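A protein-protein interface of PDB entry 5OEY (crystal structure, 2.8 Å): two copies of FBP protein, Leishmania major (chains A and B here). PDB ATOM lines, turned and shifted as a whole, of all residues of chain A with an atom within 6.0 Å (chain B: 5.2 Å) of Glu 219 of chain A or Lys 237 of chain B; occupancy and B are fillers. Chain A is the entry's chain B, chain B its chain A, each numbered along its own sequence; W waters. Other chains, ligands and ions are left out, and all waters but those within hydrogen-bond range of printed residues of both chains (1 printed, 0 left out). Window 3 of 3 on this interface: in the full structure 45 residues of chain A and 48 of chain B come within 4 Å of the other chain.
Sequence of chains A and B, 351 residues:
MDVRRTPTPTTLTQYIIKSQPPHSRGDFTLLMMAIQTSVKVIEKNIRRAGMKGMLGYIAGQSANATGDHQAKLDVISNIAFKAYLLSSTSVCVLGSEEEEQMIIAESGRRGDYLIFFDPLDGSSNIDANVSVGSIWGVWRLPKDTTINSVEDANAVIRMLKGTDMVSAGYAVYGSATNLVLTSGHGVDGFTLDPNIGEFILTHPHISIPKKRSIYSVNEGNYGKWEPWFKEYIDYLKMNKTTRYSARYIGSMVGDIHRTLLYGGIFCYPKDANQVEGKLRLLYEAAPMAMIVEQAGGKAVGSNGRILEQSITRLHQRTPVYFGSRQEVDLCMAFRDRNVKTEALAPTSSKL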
ATOM      1  N   TYR A 215     -33.336  16.529 -41.823  1.00  0.00           N
ATOM      2  CA  TYR A 215     -32.155  17.316 -41.486  1.00  0.00           C
ATOM      3  C   TYR A 215     -31.212  16.460 -40.667  1.00  0.00           C
ATOM      4  O   TYR A 215     -31.638  15.617 -39.841  1.00  0.00           O
ATOM      5  CB  TYR A 215     -32.500  18.635 -40.767  1.00  0.00           C
ATOM      6  CG  TYR A 215     -32.958  18.516 -39.319  1.00  0.00           C
ATOM      7  CD1 TYR A 215     -34.270  18.175 -39.008  1.00  0.00           C
ATOM      8  CD2 TYR A 215     -32.098  18.793 -38.264  1.00  0.00           C
ATOM      9  CE1 TYR A 215     -34.698  18.096 -37.700  1.00  0.00           C
ATOM     10  CE2 TYR A 215     -32.515  18.714 -36.938  1.00  0.00           C
ATOM     11  CZ  TYR A 215     -33.811  18.359 -36.662  1.00  0.00           C
ATOM     12  OH  TYR A 215     -34.270  18.254 -35.368  1.00  0.00           O
ATOM     13  N   VAL A 217     -27.641  16.836 -38.411  1.00  0.00           N
ATOM     14  CA  VAL A 217     -26.721  17.692 -37.685  1.00  0.00           C
ATOM     15  C   VAL A 217     -26.576  17.141 -36.261  1.00  0.00           C
ATOM     16  O   VAL A 217     -27.497  16.482 -35.767  1.00  0.00           O
ATOM     17  CB  VAL A 217     -27.239  19.165 -37.683  1.00  0.00           C
ATOM     18  CG1 VAL A 217     -28.479  19.322 -36.813  1.00  0.00           C
ATOM     19  CG2 VAL A 217     -26.148  20.128 -37.248  1.00  0.00           C
ATOM     20  N   ASN A 218     -25.440  17.403 -35.605  1.00  0.00           N
ATOM     21  CA  ASN A 218     -25.279  17.075 -34.175  1.00  0.00           C
ATOM     22  C   ASN A 218     -25.879  18.146 -33.236  1.00  0.00           C
ATOM     23  O   ASN A 218     -25.208  19.130 -32.900  1.00  0.00           O
ATOM     24  CB  ASN A 218     -23.814  16.883 -33.851  1.00  0.00           C
ATOM     25  CG  ASN A 218     -23.578  16.468 -32.418  1.00  0.00           C
ATOM     26  OD1 ASN A 218     -24.495  16.306 -31.618  1.00  0.00           O
ATOM     27  ND2 ASN A 218     -22.335  16.236 -32.106  1.00  0.00           N
ATOM     28  N   GLU A 219     -27.124  17.923 -32.785  1.00  0.00           N
ATOM     29  CA  GLU A 219     -27.805  18.907 -31.930  1.00  0.00           C
ATOM     30  C   GLU A 219     -27.272  18.938 -30.507  1.00  0.00           C
ATOM     31  O   GLU A 219     -27.625  19.827 -29.732  1.00  0.00           O
ATOM     32  CB  GLU A 219     -29.311  18.698 -31.912  1.00  0.00           C
ATOM     33  CG  GLU A 219     -29.974  19.000 -33.242  1.00  0.00           C
ATOM     34  CD  GLU A 219     -31.488  19.122 -33.130  1.00  0.00           C
ATOM     35  OE1 GLU A 219     -31.945  20.031 -32.408  1.00  0.00           O
ATOM     36  OE2 GLU A 219     -32.214  18.321 -33.788  1.00  0.00           O
ATOM     37  N   GLY A 220     -26.407  17.994 -30.164  1.00  0.00           N
ATOM     38  CA  GLY A 220     -25.650  18.067 -28.929  1.00  0.00           C
ATOM     39  C   GLY A 220     -24.875  19.360 -28.793  1.00  0.00           C
ATOM     40  O   GLY A 220     -24.733  19.863 -27.679  1.00  0.00           O
ATOM     41  N   ASN A 221     -24.411  19.898 -29.928  1.00  0.00           N
ATOM     42  CA  ASN A 221     -23.711  21.202 -30.000  1.00  0.00           C
ATOM     43  C   ASN A 221     -24.586  22.456 -30.109  1.00  0.00           C
ATOM     44  O   ASN A 221     -24.066  23.514 -30.435  1.00  0.00           O
ATOM     45  CB  ASN A 221     -22.791  21.255 -31.232  1.00  0.00           C
ATOM     46  CG  ASN A 221     -21.679  20.255 -31.183  1.00  0.00           C
ATOM     47  OD1 ASN A 221     -21.082  20.032 -30.145  1.00  0.00           O
ATOM     48  ND2 ASN A 221     -21.396  19.636 -32.318  1.00  0.00           N
ATOM     49  N   TYR A 222     -25.891  22.354 -29.876  1.00  0.00           N
ATOM     50  CA  TYR A 222     -26.785  23.516 -29.998  1.00  0.00           C
ATOM     51  C   TYR A 222     -26.188  24.781 -29.401  1.00  0.00           C
ATOM     52  O   TYR A 222     -25.999  25.759 -30.103  1.00  0.00           O
ATOM     53  CB  TYR A 222     -28.113  23.229 -29.325  1.00  0.00           C
ATOM     54  CG  TYR A 222     -29.167  24.275 -29.555  1.00  0.00           C
ATOM     55  CD1 TYR A 222     -29.984  24.247 -30.688  1.00  0.00           C
ATOM     56  CD2 TYR A 222     -29.389  25.284 -28.607  1.00  0.00           C
ATOM     57  CE1 TYR A 222     -30.981  25.206 -30.880  1.00  0.00           C
ATOM     58  CE2 TYR A 222     -30.382  26.244 -28.795  1.00  0.00           C
ATOM     59  CZ  TYR A 222     -31.171  26.198 -29.937  1.00  0.00           C
ATOM     60  OH  TYR A 222     -32.157  27.132 -30.105  1.00  0.00           O
ATOM     61  N   GLY A 223     -25.821  24.706 -28.131  1.00  0.00           N
ATOM     62  CA  GLY A 223     -25.273  25.836 -27.389  1.00  0.00           C
ATOM     63  C   GLY A 223     -24.126  26.599 -28.014  1.00  0.00           C
ATOM     64  O   GLY A 223     -24.020  27.805 -27.818  1.00  0.00           O
ATOM     65  N   TRP A 225     -23.497  26.892 -31.368  1.00  0.00           N
ATOM     66  CA  TRP A 225     -23.800  27.357 -32.712  1.00  0.00           C
ATOM     67  C   TRP A 225     -24.008  28.862 -32.766  1.00  0.00           C
ATOM     68  O   TRP A 225     -24.263  29.503 -31.745  1.00  0.00           O
ATOM     69  CB  TRP A 225     -25.072  26.688 -33.221  1.00  0.00           C
ATOM     70  CG  TRP A 225     -24.975  25.231 -33.462  1.00  0.00           C
ATOM     71  CD1 TRP A 225     -23.855  24.495 -33.672  1.00  0.00           C
ATOM     72  CD2 TRP A 225     -26.073  24.337 -33.611  1.00  0.00           C
ATOM     73  NE1 TRP A 225     -24.191  23.187 -33.898  1.00  0.00           N
ATOM     74  CE2 TRP A 225     -25.548  23.070 -33.873  1.00  0.00           C
ATOM     75  CE3 TRP A 225     -27.460  24.486 -33.529  1.00  0.00           C
ATOM     76  CZ2 TRP A 225     -26.352  21.954 -34.029  1.00  0.00           C
ATOM     77  CZ3 TRP A 225     -28.263  23.375 -33.692  1.00  0.00           C
ATOM     78  CH2 TRP A 225     -27.708  22.128 -33.938  1.00  0.00           C
ATOM     79  N   ILE A 233     -32.686  25.701 -37.087  1.00  0.00           N
ATOM     80  CA  ILE A 233     -33.020  24.402 -36.514  1.00  0.00           C
ATOM     81  C   ILE A 233     -34.332  24.459 -35.750  1.00  0.00           C
ATOM     82  O   ILE A 233     -35.170  23.570 -35.904  1.00  0.00           O
ATOM     83  CB  ILE A 233     -31.859  23.818 -35.664  1.00  0.00           C
ATOM     84  CG1 ILE A 233     -30.633  23.516 -36.556  1.00  0.00           C
ATOM     85  CG2 ILE A 233     -32.272  22.543 -34.918  1.00  0.00           C
ATOM     86  CD1 ILE A 233     -30.840  22.534 -37.703  1.00  0.00           C
ATOM     87  N   LYS A 237     -38.172  22.473 -36.475  1.00  0.00           N
ATOM     88  CA  LYS A 237     -38.973  21.803 -35.477  1.00  0.00           C
ATOM     89  C   LYS A 237     -40.310  22.434 -35.175  1.00  0.00           C
ATOM     90  O   LYS A 237     -41.235  21.718 -34.799  1.00  0.00           O
ATOM     91  CB  LYS A 237     -38.221  21.772 -34.179  1.00  0.00           C
ATOM     92  CG  LYS A 237     -36.902  21.055 -34.259  1.00  0.00           C
ATOM     93  CD  LYS A 237     -36.258  21.160 -32.907  1.00  0.00           C
ATOM     94  CE  LYS A 237     -34.945  20.453 -32.886  1.00  0.00           C
ATOM     95  NZ  LYS A 237     -34.455  20.575 -31.496  1.00  0.00           N
ATOM     96  N   ALA A 246     -35.389  13.914 -38.204  1.00  0.00           N
ATOM     97  CA  ALA A 246     -33.978  14.097 -37.877  1.00  0.00           C
ATOM     98  C   ALA A 246     -33.255  12.775 -37.965  1.00  0.00           C
ATOM     99  O   ALA A 246     -33.734  11.772 -37.448  1.00  0.00           O
ATOM    100  CB  ALA A 246     -33.812  14.684 -36.488  1.00  0.00           C
ATOM    101  N   TYR A 248     -29.021  11.512 -37.756  1.00  0.00           N
ATOM    102  CA  TYR A 248     -27.568  11.766 -37.661  1.00  0.00           C
ATOM    103  C   TYR A 248     -26.830  10.486 -37.226  1.00  0.00           C
ATOM    104  O   TYR A 248     -26.800  10.129 -36.043  1.00  0.00           O
ATOM    105  CB  TYR A 248     -27.301  12.936 -36.717  1.00  0.00           C
ATOM    106  CG  TYR A 248     -25.904  13.503 -36.784  1.00  0.00           C
ATOM    107  CD1 TYR A 248     -25.466  14.197 -37.902  1.00  0.00           C
ATOM    108  CD2 TYR A 248     -25.002  13.342 -35.723  1.00  0.00           C
ATOM    109  CE1 TYR A 248     -24.181  14.703 -37.968  1.00  0.00           C
ATOM    110  CE2 TYR A 248     -23.708  13.843 -35.783  1.00  0.00           C
ATOM    111  CZ  TYR A 248     -23.306  14.534 -36.900  1.00  0.00           C
ATOM    112  OH  TYR A 248     -22.051  15.084 -36.960  1.00  0.00           O
ATOM    113  N   TYR B 215     -26.904  11.137 -26.267  1.00  0.00           N
ATOM    114  CA  TYR B 215     -28.339  10.941 -26.283  1.00  0.00           C
ATOM    115  C   TYR B 215     -28.792  10.660 -27.700  1.00  0.00           C
ATOM    116  O   TYR B 215     -28.242  11.222 -28.681  1.00  0.00           O
ATOM    117  CB  TYR B 215     -29.099  12.130 -25.653  1.00  0.00           C
ATOM    118  CG  TYR B 215     -29.157  13.407 -26.475  1.00  0.00           C
ATOM    119  CD1 TYR B 215     -28.105  14.275 -26.509  1.00  0.00           C
ATOM    120  CD2 TYR B 215     -30.301  13.746 -27.208  1.00  0.00           C
ATOM    121  CE1 TYR B 215     -28.165  15.448 -27.259  1.00  0.00           C
ATOM    122  CE2 TYR B 215     -30.366  14.905 -27.967  1.00  0.00           C
ATOM    123  CZ  TYR B 215     -29.297  15.760 -27.987  1.00  0.00           C
ATOM    124  OH  TYR B 215     -29.324  16.943 -28.704  1.00  0.00           O
ATOM    125  N   GLU B 219     -35.189  14.361 -32.777  1.00  0.00           N
ATOM    126  CA  GLU B 219     -35.570  15.734 -32.399  1.00  0.00           C
ATOM    127  C   GLU B 219     -36.458  16.444 -33.431  1.00  0.00           C
ATOM    128  O   GLU B 219     -36.977  17.529 -33.160  1.00  0.00           O
ATOM    129  CB  GLU B 219     -34.345  16.591 -32.084  1.00  0.00           C
ATOM    130  CG  GLU B 219     -33.599  16.141 -30.835  1.00  0.00           C
ATOM    131  CD  GLU B 219     -32.602  17.159 -30.337  1.00  0.00           C
ATOM    132  OE1 GLU B 219     -33.055  18.282 -29.985  1.00  0.00           O
ATOM    133  OE2 GLU B 219     -31.380  16.846 -30.291  1.00  0.00           O
ATOM    134  N   GLY B 220     -36.633  15.838 -34.603  1.00  0.00           N
ATOM    135  CA  GLY B 220     -37.644  16.278 -35.554  1.00  0.00           C
ATOM    136  C   GLY B 220     -39.045  16.355 -34.960  1.00  0.00           C
ATOM    137  O   GLY B 220     -39.794  17.268 -35.300  1.00  0.00           O
ATOM    138  N   ILE B 233     -34.369  17.324 -22.788  1.00  0.00           N
ATOM    139  CA  ILE B 233     -33.537  17.497 -23.971  1.00  0.00           C
ATOM    140  C   ILE B 233     -32.858  18.864 -23.993  1.00  0.00           C
ATOM    141  O   ILE B 233     -31.659  18.952 -24.265  1.00  0.00           O
ATOM    142  CB  ILE B 233     -34.321  17.211 -25.279  1.00  0.00           C
ATOM    143  CG1 ILE B 233     -34.759  15.726 -25.336  1.00  0.00           C
ATOM    144  CG2 ILE B 233     -33.495  17.550 -26.529  1.00  0.00           C
ATOM    145  CD1 ILE B 233     -33.650  14.685 -25.260  1.00  0.00           C
ATOM    146  N   ASP B 234     -33.603  19.920 -23.683  1.00  0.00           N
ATOM    147  CA  ASP B 234     -33.016  21.264 -23.572  1.00  0.00           C
ATOM    148  C   ASP B 234     -31.884  21.340 -22.533  1.00  0.00           C
ATOM    149  O   ASP B 234     -30.860  21.982 -22.780  1.00  0.00           O
ATOM    150  CB  ASP B 234     -34.094  22.306 -23.250  1.00  0.00           C
ATOM    151  CG  ASP B 234     -35.016  22.608 -24.440  1.00  0.00           C
ATOM    152  OD1 ASP B 234     -34.766  22.132 -25.573  1.00  0.00           O
ATOM    153  OD2 ASP B 234     -36.001  23.339 -24.205  1.00  0.00           O
ATOM    154  N   TYR B 235     -32.070  20.671 -21.388  1.00  0.00           N
ATOM    155  CA  TYR B 235     -31.032  20.574 -20.349  1.00  0.00           C
ATOM    156  C   TYR B 235     -29.776  19.909 -20.881  1.00  0.00           C
ATOM    157  O   TYR B 235     -28.681  20.400 -20.646  1.00  0.00           O
ATOM    158  CB  TYR B 235     -31.537  19.829 -19.100  1.00  0.00           C
ATOM    159  CG  TYR B 235     -30.484  19.695 -18.000  1.00  0.00           C
ATOM    160  CD1 TYR B 235     -30.218  20.745 -17.128  1.00  0.00           C
ATOM    161  CD2 TYR B 235     -29.753  18.514 -17.843  1.00  0.00           C
ATOM    162  CE1 TYR B 235     -29.261  20.627 -16.124  1.00  0.00           C
ATOM    163  CE2 TYR B 235     -28.788  18.395 -16.847  1.00  0.00           C
ATOM    164  CZ  TYR B 235     -28.546  19.455 -15.988  1.00  0.00           C
ATOM    165  OH  TYR B 235     -27.593  19.348 -15.007  1.00  0.00           O
ATOM    166  N   LEU B 236     -29.926  18.809 -21.624  1.00  0.00           N
ATOM    167  CA  LEU B 236     -28.756  18.133 -22.199  1.00  0.00           C
ATOM    168  C   LEU B 236     -27.947  19.067 -23.090  1.00  0.00           C
ATOM    169  O   LEU B 236     -26.738  18.953 -23.167  1.00  0.00           O
ATOM    170  CB  LEU B 236     -29.150  16.876 -22.979  1.00  0.00           C
ATOM    171  CG  LEU B 236     -29.868  15.741 -22.252  1.00  0.00           C
ATOM    172  CD1 LEU B 236     -30.137  14.637 -23.251  1.00  0.00           C
ATOM    173  CD2 LEU B 236     -29.095  15.221 -21.056  1.00  0.00           C
ATOM    174  N   LYS B 237     -28.620  19.993 -23.750  1.00  0.00           N
ATOM    175  CA  LYS B 237     -27.959  20.954 -24.618  1.00  0.00           C
ATOM    176  C   LYS B 237     -27.480  22.218 -23.963  1.00  0.00           C
ATOM    177  O   LYS B 237     -26.476  22.772 -24.396  1.00  0.00           O
ATOM    178  CB  LYS B 237     -28.918  21.413 -25.686  1.00  0.00           C
ATOM    179  CG  LYS B 237     -29.437  20.310 -26.571  1.00  0.00           C
ATOM    180  CD  LYS B 237     -30.410  20.933 -27.513  1.00  0.00           C
ATOM    181  CE  LYS B 237     -30.956  19.902 -28.442  1.00  0.00           C
ATOM    182  NZ  LYS B 237     -31.842  20.636 -29.375  1.00  0.00           N
ATOM    183  N   MET B 238     -28.220  22.708 -22.967  1.00  0.00           N
ATOM    184  CA  MET B 238     -27.963  24.034 -22.398  1.00  0.00           C
ATOM    185  C   MET B 238     -27.280  24.048 -21.016  1.00  0.00           C
ATOM    186  O   MET B 238     -26.851  25.108 -20.587  1.00  0.00           O
ATOM    187  CB  MET B 238     -29.275  24.854 -22.326  1.00  0.00           C
ATOM    188  CG  MET B 238     -30.048  25.036 -23.655  1.00  0.00           C
ATOM    189  SD  MET B 238     -29.202  25.874 -24.998  1.00  0.00           S
ATOM    190  CE  MET B 238     -28.772  27.468 -24.273  1.00  0.00           C
ATOM    191  N   ASN B 239     -27.167  22.904 -20.325  1.00  0.00           N
ATOM    192  CA  ASN B 239     -26.577  22.858 -18.967  1.00  0.00           C
ATOM    193  C   ASN B 239     -25.100  23.292 -18.972  1.00  0.00           C
ATOM    194  O   ASN B 239     -24.385  23.067 -19.946  1.00  0.00           O
ATOM    195  CB  ASN B 239     -26.730  21.470 -18.327  1.00  0.00           C
ATOM    196  CG  ASN B 239     -25.675  20.475 -18.811  1.00  0.00           C
ATOM    197  OD1 ASN B 239     -24.624  20.326 -18.179  1.00  0.00           O
ATOM    198  ND2 ASN B 239     -25.944  19.800 -19.932  1.00  0.00           N
ATOM    199  N   ARG B 243     -21.134  18.344 -21.436  1.00  0.00           N
ATOM    200  CA  ARG B 243     -21.516  18.478 -22.839  1.00  0.00           C
ATOM    201  C   ARG B 243     -21.979  17.159 -23.356  1.00  0.00           C
ATOM    202  O   ARG B 243     -21.315  16.144 -23.164  1.00  0.00           O
ATOM    203  CB  ARG B 243     -20.333  18.942 -23.687  1.00  0.00           C
ATOM    204  CG  ARG B 243     -19.986  20.430 -23.569  1.00  0.00           C
ATOM    205  CD  ARG B 243     -21.028  21.348 -24.239  1.00  0.00           C
ATOM    206  NE  ARG B 243     -22.380  21.513 -23.714  1.00  0.00           N
ATOM    207  CZ  ARG B 243     -22.757  21.971 -22.527  1.00  0.00           C
ATOM    208  NH1 ARG B 243     -21.892  22.319 -21.576  1.00  0.00           N
ATOM    209  NH2 ARG B 243     -24.075  22.054 -22.291  1.00  0.00           N
ATOM    210  N   ALA B 246     -25.004  14.105 -29.679  1.00  0.00           N
ATOM    211  CA  ALA B 246     -26.243  13.532 -30.218  1.00  0.00           C
ATOM    212  C   ALA B 246     -25.953  12.565 -31.360  1.00  0.00           C
ATOM    213  O   ALA B 246     -25.168  12.874 -32.257  1.00  0.00           O
ATOM    214  CB  ALA B 246     -27.160  14.626 -30.709  1.00  0.00           C
HETATM  215  O   HOH W   1     -41.408  19.042 -34.070  1.00  0.00           O
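Water W1 lies within hydrogen-bond range of O of Gly 220 of chain B (2.7 Å) and O of Lys 237 of chain A (2.8 Å).
The side-chain carboxylate of Glu 219 of chain B is in salt-bridge range of the side-chain amino group of Lys 237 of chain A (3.1 Å). The side-chain carboxylate (OE1) of Glu 219 of chain B lies close to the side-chain carboxylate (OE1) of Glu 219 of chain A, at 3.2 Å. The side-chain hydroxyl of Tyr 215 of chain A sits at hydrogen-bond distance from the backbone NH of Gly 220 of chain B, at 3.5 Å. N of Gly 220 of chain A lies within hydrogen-bond range of OH of Tyr 215 of chain B (3.4 Å). N of Ala 246 of chain B lies within hydrogen-bond range of OD1 of Asn 218 of chain A (3.0 Å). NZ of Lys 237 of chain B is in salt-bridge range of OE1 of Glu 219 of chain A (3.1 Å). NZ of Lys 237 of chain A sits close to NZ of Lys 237 of chain B, 3.4 Å away.
Tyr 215 of chain A touches Glu 219 of chain B, and with the chains exchanged Glu 219 of chain A touches Tyr 215 of chain B. Glu 219 of chain B touches its own counterpart, Glu 219 of chain A. Gly 220 of chain A touches Ala 246 of chain B, and with the chains exchanged Ala 246 of chain A touches Gly 220 of chain B. Lys 237 of chain B touches its own counterpart, Lys 237 of chain A. Of the 16 pairs that touch across the chains among the printed residues, 12 have their exchanged pair printed and touching as well.
C of Glu 219 of chain B touches OH of Tyr 215 of chain A, 3.4 Å away. Glu 219 of chain A touches Tyr 215 of chain B. CB of Ala 246 of chain B touches N of Glu 219 of chain A, 3.9 Å away. Gly 220 of chain A touches Ala 246 of chain B (N to CB, 3.5 Å). CB of Tyr 222 of chain A touches CD of Lys 237 of chain B (3.7 Å). Tyr 222 of chain A touches Met 238 of chain B (CD2 to SD, 3.7 Å). Glu 219 of chain B touches Ala 246 of chain A. N of Gly 220 of chain B touches CB of Ala 246 of chain A, at 3.6 Å. O of Ala 246 of chain B touches CD2 of Tyr 248 of chain A, 3.5 Å away.
The side-chain carboxylate (OE2) of Glu 219 of chain B lies within hydrogen-bond range of the side-chain hydroxyl (OH) of Tyr 215 of chain B (2.6 Å). The backbone NH (N) of Gly 220 of chain A is in hydrogen-bond range of the side-chain amide oxygen (OD1) of Asn 218 of chain A. The side-chain hydroxyl of Tyr 215 of chain A is in hydrogen-bond range of the side-chain carboxylate of Glu 219 of chain A (2.6 Å). The backbone carbonyl oxygen of Lys 237 of chain B sits at hydrogen-bond distance from the guanidinium group of Arg 243 of chain B, at 3.3 Å. The side-chain carboxylate (OE1) of Glu 219 of chain B is in salt-bridge range of the side-chain amino group (NZ) of Lys 237 of chain B (2.7 Å). NZ of Lys 237 of chain A is in salt-bridge range of OE1 of Glu 219 of chain A, at 2.7 Å.
Of the printed residues of chain B, Asn 218 of chain A touches Ala 246 (3.0 Å). Ile 233 of chain A touches none of the printed residues of chain B. Of the printed residues of chain B, Lys 237 of chain A touches Glu 219 (3.1 Å) and Lys 237 (3.4 Å). Of chain A, only Glu 219 (3.1 Å), Tyr 222 (3.7 Å) and Lys 237 (3.4 Å) come within 4 Å of Lys 237 of chain B. Arg 243 of chain B touches none of the printed residues of chain A. Printed residues of chain A within 4 Å of Ala 246 of chain B: Asn 218, Glu 219, Gly 220 and Tyr 248. The nearest residue of chain B that does not touch Glu 219 of chain A is Gly 220 of chain B (5.1 Å). The nearest printed residue of chain A that does not touch Tyr 215 of chain B is Asn 218 of chain A (5.7 Å).
Printed residues of chain B that touch a printed residue of chain A: Tyr 215, Glu 219, Gly 220, Lys 237, Met 238 and Ala 246. Hydrophobic or aromatic side chains of chain B within 4 Å of the printed part of chain A: Tyr 215, Met 238 and Ala 246. Of the 13 printed residues of chain A, 8 touch a printed residue of chain B. Printed residues of chain A that touch a printed residue of chain B: Tyr 215, Asn 218, Glu 219, Gly 220, Tyr 222, Lys 237, Ala 246 and Tyr 248. Hydrophobic or aromatic side chains of chain A within 4 Å of the printed part of chain B: Tyr 215, Tyr 222, Ala 246 and Tyr 248. Among the printed residues, 16 pairs touch across the chains. Among the printed residues, Asp or Glu carboxylates within 4 Å of a Lys or Arg side-chain nitrogen of the other chain: Glu 219 of chain A with Lys 237 of chain B and Lys 237 of chain A with Glu 219 of chain B.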
